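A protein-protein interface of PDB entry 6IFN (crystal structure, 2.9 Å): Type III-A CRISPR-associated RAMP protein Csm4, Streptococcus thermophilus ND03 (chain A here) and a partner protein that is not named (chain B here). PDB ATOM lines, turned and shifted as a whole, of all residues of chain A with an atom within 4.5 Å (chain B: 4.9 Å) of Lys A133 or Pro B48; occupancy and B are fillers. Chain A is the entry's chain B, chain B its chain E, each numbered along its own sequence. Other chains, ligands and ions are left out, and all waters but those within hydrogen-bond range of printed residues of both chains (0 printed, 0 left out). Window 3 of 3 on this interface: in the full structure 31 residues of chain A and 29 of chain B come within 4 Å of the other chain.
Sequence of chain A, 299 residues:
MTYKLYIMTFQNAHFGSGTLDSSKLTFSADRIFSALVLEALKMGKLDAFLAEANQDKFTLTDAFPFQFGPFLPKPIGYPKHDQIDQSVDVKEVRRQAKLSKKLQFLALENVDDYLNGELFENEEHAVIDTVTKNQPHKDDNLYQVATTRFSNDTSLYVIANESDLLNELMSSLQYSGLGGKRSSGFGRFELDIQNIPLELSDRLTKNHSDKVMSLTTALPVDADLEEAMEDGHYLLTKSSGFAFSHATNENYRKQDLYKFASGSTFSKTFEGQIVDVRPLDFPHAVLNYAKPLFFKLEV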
ATOM      1  N   VAL A 131     -29.268  15.122  20.570  1.00  0.00           N
ATOM      2  CA  VAL A 131     -29.285  16.564  20.489  1.00  0.00           C
ATOM      3  C   VAL A 131     -30.705  16.980  20.131  1.00  0.00           C
ATOM      4  O   VAL A 131     -31.422  16.273  19.492  1.00  0.00           O
ATOM      5  CB  VAL A 131     -28.276  17.127  19.473  1.00  0.00           C
ATOM      6  CG1 VAL A 131     -26.902  16.496  19.635  1.00  0.00           C
ATOM      7  CG2 VAL A 131     -28.768  16.984  18.041  1.00  0.00           C
ATOM      8  N   THR A 132     -31.088  18.151  20.607  1.00  0.00           N
ATOM      9  CA  THR A 132     -32.340  18.708  20.327  1.00  0.00           C
ATOM     10  C   THR A 132     -32.168  19.633  19.138  1.00  0.00           C
ATOM     11  O   THR A 132     -31.250  20.431  19.118  1.00  0.00           O
ATOM     12  CB  THR A 132     -32.875  19.470  21.536  1.00  0.00           C
ATOM     13  OG1 THR A 132     -33.439  18.474  22.384  1.00  0.00           O
ATOM     14  CG2 THR A 132     -33.913  20.504  21.171  1.00  0.00           C
ATOM     15  N   LYS A 133     -33.078  19.501  18.180  1.00  0.00           N
ATOM     16  CA  LYS A 133     -33.191  20.396  17.049  1.00  0.00           C
ATOM     17  C   LYS A 133     -34.600  20.997  17.082  1.00  0.00           C
ATOM     18  O   LYS A 133     -35.508  20.464  17.759  1.00  0.00           O
ATOM     19  CB  LYS A 133     -32.922  19.627  15.746  1.00  0.00           C
ATOM     20  CG  LYS A 133     -31.510  19.052  15.591  1.00  0.00           C
ATOM     21  CD  LYS A 133     -31.428  17.903  14.611  1.00  0.00           C
ATOM     22  CE  LYS A 133     -30.158  17.097  14.733  1.00  0.00           C
ATOM     23  NZ  LYS A 133     -28.999  17.853  14.209  1.00  0.00           N
ATOM     24  N   ASN A 134     -34.777  22.097  16.344  1.00  0.00           N
ATOM     25  CA  ASN A 134     -36.063  22.754  16.260  1.00  0.00           C
ATOM     26  C   ASN A 134     -36.383  23.067  14.809  1.00  0.00           C
ATOM     27  O   ASN A 134     -35.530  22.945  13.936  1.00  0.00           O
ATOM     28  CB  ASN A 134     -36.113  24.082  17.005  1.00  0.00           C
ATOM     29  CG  ASN A 134     -35.568  25.245  16.196  1.00  0.00           C
ATOM     30  OD1 ASN A 134     -34.670  25.079  15.364  1.00  0.00           O
ATOM     31  ND2 ASN A 134     -36.107  26.436  16.449  1.00  0.00           N
ATOM     32  N   LEU A 142     -40.229  20.592  18.345  1.00  0.00           N
ATOM     33  CA  LEU A 142     -38.960  20.551  19.054  1.00  0.00           C
ATOM     34  C   LEU A 142     -38.680  19.070  19.299  1.00  0.00           C
ATOM     35  O   LEU A 142     -39.519  18.407  19.859  1.00  0.00           O
ATOM     36  CB  LEU A 142     -39.098  21.306  20.376  1.00  0.00           C
ATOM     37  CG  LEU A 142     -37.798  21.868  20.941  1.00  0.00           C
ATOM     38  CD1 LEU A 142     -37.355  23.100  20.168  1.00  0.00           C
ATOM     39  CD2 LEU A 142     -37.947  22.194  22.424  1.00  0.00           C
ATOM     40  N   TYR A 143     -37.563  18.531  18.814  1.00  0.00           N
ATOM     41  CA  TYR A 143     -37.363  17.082  18.926  1.00  0.00           C
ATOM     42  C   TYR A 143     -35.898  16.753  19.164  1.00  0.00           C
ATOM     43  O   TYR A 143     -35.030  17.613  18.980  1.00  0.00           O
ATOM     44  CB  TYR A 143     -37.840  16.359  17.673  1.00  0.00           C
ATOM     45  CG  TYR A 143     -37.047  16.649  16.428  1.00  0.00           C
ATOM     46  CD1 TYR A 143     -37.306  17.774  15.664  1.00  0.00           C
ATOM     47  CD2 TYR A 143     -36.051  15.787  15.998  1.00  0.00           C
ATOM     48  CE1 TYR A 143     -36.587  18.042  14.510  1.00  0.00           C
ATOM     49  CE2 TYR A 143     -35.319  16.040  14.849  1.00  0.00           C
ATOM     50  CZ  TYR A 143     -35.594  17.169  14.096  1.00  0.00           C
ATOM     51  OH  TYR A 143     -34.890  17.419  12.948  1.00  0.00           O
ATOM     52  N   VAL A 145     -32.831  13.849  18.433  1.00  0.00           N
ATOM     53  CA  VAL A 145     -32.355  12.753  17.692  1.00  0.00           C
ATOM     54  C   VAL A 145     -31.057  12.314  18.358  1.00  0.00           C
ATOM     55  O   VAL A 145     -30.215  13.119  18.637  1.00  0.00           O
ATOM     56  CB  VAL A 145     -32.194  13.057  16.190  1.00  0.00           C
ATOM     57  CG1 VAL A 145     -31.421  14.320  15.918  1.00  0.00           C
ATOM     58  CG2 VAL A 145     -31.530  11.911  15.466  1.00  0.00           C
ATOM     59  N   PHE A 186     -26.753  12.237   8.876  1.00  0.00           N
ATOM     60  CA  PHE A 186     -26.153  11.047   9.506  1.00  0.00           C
ATOM     61  C   PHE A 186     -25.871   9.949   8.474  1.00  0.00           C
ATOM     62  O   PHE A 186     -26.170  10.090   7.270  1.00  0.00           O
ATOM     63  CB  PHE A 186     -27.005  10.630  10.707  1.00  0.00           C
ATOM     64  CG  PHE A 186     -27.301  11.776  11.660  1.00  0.00           C
ATOM     65  CD1 PHE A 186     -26.274  12.552  12.199  1.00  0.00           C
ATOM     66  CD2 PHE A 186     -28.598  12.105  12.003  1.00  0.00           C
ATOM     67  CE1 PHE A 186     -26.533  13.610  13.055  1.00  0.00           C
ATOM     68  CE2 PHE A 186     -28.857  13.168  12.851  1.00  0.00           C
ATOM     69  CZ  PHE A 186     -27.829  13.909  13.384  1.00  0.00           C
ATOM     70  N   ILE B  20     -24.605  28.097  16.800  1.00  0.00           N
ATOM     71  CA  ILE B  20     -25.716  27.215  16.525  1.00  0.00           C
ATOM     72  C   ILE B  20     -26.340  26.717  17.842  1.00  0.00           C
ATOM     73  O   ILE B  20     -27.440  27.147  18.220  1.00  0.00           O
ATOM     74  CB  ILE B  20     -25.296  26.113  15.551  1.00  0.00           C
ATOM     75  CG1 ILE B  20     -24.903  26.721  14.197  1.00  0.00           C
ATOM     76  CG2 ILE B  20     -26.405  25.097  15.400  1.00  0.00           C
ATOM     77  CD1 ILE B  20     -24.635  25.725  13.064  1.00  0.00           C
ATOM     78  N   ILE B  37     -23.212  24.145  19.602  1.00  0.00           N
ATOM     79  CA  ILE B  37     -23.252  22.676  19.381  1.00  0.00           C
ATOM     80  C   ILE B  37     -21.826  22.223  19.035  1.00  0.00           C
ATOM     81  O   ILE B  37     -21.156  22.839  18.200  1.00  0.00           O
ATOM     82  CB  ILE B  37     -24.270  22.236  18.311  1.00  0.00           C
ATOM     83  CG1 ILE B  37     -24.317  20.710  18.235  1.00  0.00           C
ATOM     84  CG2 ILE B  37     -23.947  22.839  16.958  1.00  0.00           C
ATOM     85  CD1 ILE B  37     -25.411  20.143  17.355  1.00  0.00           C
ATOM     86  N   ILE B  46     -19.144  22.128  15.584  1.00  0.00           N
ATOM     87  CA  ILE B  46     -19.590  21.297  14.483  1.00  0.00           C
ATOM     88  C   ILE B  46     -20.735  22.049  13.828  1.00  0.00           C
ATOM     89  O   ILE B  46     -21.458  22.768  14.506  1.00  0.00           O
ATOM     90  CB  ILE B  46     -20.009  19.915  15.008  1.00  0.00           C
ATOM     91  CG1 ILE B  46     -20.300  18.920  13.892  1.00  0.00           C
ATOM     92  CG2 ILE B  46     -21.170  20.030  15.978  1.00  0.00           C
ATOM     93  CD1 ILE B  46     -20.783  17.577  14.415  1.00  0.00           C
ATOM     94  N   ILE B  47     -20.833  21.935  12.508  1.00  0.00           N
ATOM     95  CA  ILE B  47     -21.951  22.497  11.779  1.00  0.00           C
ATOM     96  C   ILE B  47     -22.879  21.346  11.433  1.00  0.00           C
ATOM     97  O   ILE B  47     -22.602  20.597  10.510  1.00  0.00           O
ATOM     98  CB  ILE B  47     -21.493  23.249  10.513  1.00  0.00           C
ATOM     99  CG1 ILE B  47     -20.616  24.458  10.865  1.00  0.00           C
ATOM    100  CG2 ILE B  47     -22.698  23.645   9.671  1.00  0.00           C
ATOM    101  CD1 ILE B  47     -20.238  25.306   9.684  1.00  0.00           C
ATOM    102  N   PRO B  48     -24.028  21.185  12.116  1.00  0.00           N
ATOM    103  CA  PRO B  48     -24.903  20.052  11.854  1.00  0.00           C
ATOM    104  C   PRO B  48     -25.501  20.176  10.448  1.00  0.00           C
ATOM    105  O   PRO B  48     -25.931  21.252  10.034  1.00  0.00           O
ATOM    106  CB  PRO B  48     -26.005  20.110  12.924  1.00  0.00           C
ATOM    107  CG  PRO B  48     -25.655  21.282  13.820  1.00  0.00           C
ATOM    108  CD  PRO B  48     -24.608  22.105  13.098  1.00  0.00           C
ATOM    109  N   GLY B  49     -25.528  19.052   9.728  1.00  0.00           N
ATOM    110  CA  GLY B  49     -26.155  18.977   8.402  1.00  0.00           C
ATOM    111  C   GLY B  49     -27.603  19.439   8.442  1.00  0.00           C
ATOM    112  O   GLY B  49     -28.112  19.979   7.500  1.00  0.00           O
ATOM    113  N   SER B  50     -28.278  19.183   9.556  1.00  0.00           N
ATOM    114  CA  SER B  50     -29.669  19.569   9.695  1.00  0.00           C
ATOM    115  C   SER B  50     -29.787  21.093   9.582  1.00  0.00           C
ATOM    116  O   SER B  50     -30.716  21.560   8.929  1.00  0.00           O
ATOM    117  CB  SER B  50     -30.263  19.036  10.975  1.00  0.00           C
ATOM    118  OG  SER B  50     -29.319  19.136  12.035  1.00  0.00           O
ATOM    119  N   SER B  51     -28.852  21.830  10.192  1.00  0.00           N
ATOM    120  CA  SER B  51     -28.786  23.287  10.090  1.00  0.00           C
ATOM    121  C   SER B  51     -28.670  23.723   8.624  1.00  0.00           C
ATOM    122  O   SER B  51     -29.514  24.493   8.145  1.00  0.00           O
ATOM    123  CB  SER B  51     -27.651  23.883  10.915  1.00  0.00           C
ATOM    124  OG  SER B  51     -28.033  24.046  12.271  1.00  0.00           O
ATOM    125  N   LEU B  52     -27.638  23.229   7.919  1.00  0.00           N
ATOM    126  CA  LEU B  52     -27.428  23.600   6.508  1.00  0.00           C
ATOM    127  C   LEU B  52     -28.694  23.327   5.680  1.00  0.00           C
ATOM    128  O   LEU B  52     -29.140  24.186   4.934  1.00  0.00           O
ATOM    129  CB  LEU B  52     -26.290  22.765   5.933  1.00  0.00           C
ATOM    130  CG  LEU B  52     -24.907  22.993   6.507  1.00  0.00           C
ATOM    131  CD1 LEU B  52     -24.070  21.745   6.295  1.00  0.00           C
ATOM    132  CD2 LEU B  52     -24.274  24.194   5.830  1.00  0.00           C
ATOM    133  N   ASP B 100     -22.977  16.362   8.372  1.00  0.00           N
ATOM    134  CA  ASP B 100     -22.438  17.199   9.438  1.00  0.00           C
ATOM    135  C   ASP B 100     -21.030  17.625   9.017  1.00  0.00           C
ATOM    136  O   ASP B 100     -20.229  16.797   8.620  1.00  0.00           O
ATOM    137  CB  ASP B 100     -22.415  16.501  10.803  1.00  0.00           C
ATOM    138  CG  ASP B 100     -23.780  16.260  11.443  1.00  0.00           C
ATOM    139  OD1 ASP B 100     -24.802  16.808  10.942  1.00  0.00           O
ATOM    140  OD2 ASP B 100     -23.831  15.493  12.432  1.00  0.00           O
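Of the 8 printed residues of chain A, 2 touch a printed residue of chain B.
Printed residues of chain A that touch a printed residue of chain B: Lys A133 and Phe A186.
Hydrophobic or aromatic side chains of chain A that line the printed part of chain B: Phe A186.
Of the 10 printed residues of chain B, 3 touch a printed residue of chain A.
Printed residues of chain B that touch a printed residue of chain A: Pro B48, Ser B50 and Asp B100.
Hydrophobic or aromatic side chains of chain B that line the printed part of chain A: Pro B48.
Among the printed residues, 3 pairs touch across the chains.
Among the printed residues, merely in contact across the chains: Phe A186 with Asp B100 and Lys A133 with Pro B48.
OG of Ser B50 is in hydrogen-bond range of NZ of Lys A133 (2.5 Å).
The backbone carbonyl oxygen of Tyr A143 sits at hydrogen-bond distance from the backbone NH of Lys A133, at 2.8 Å.
N of Gly B49 is in hydrogen-bond range of OD1 of Asp B100, at 2.7 Å.
Of chain B, only Pro B48 (3.96 Å) and Ser B50 (2.5 Å) come within 4 Å of Lys A133.
Asn A134 touches none of the printed residues of chain B.
Of the printed residues of chain B, Phe A186 touches Asp B100.
Of chain A, only Lys A133 (3.96 Å) comes within 4 Å of Pro B48.
Printed residues of chain A within 4 Å of Ser B50: Lys A133.
Ser B51 touches none of the printed residues of chain A.
The nearest printed residue of chain B that does not touch Lys A133 is Ile B37 (5.3 Å).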
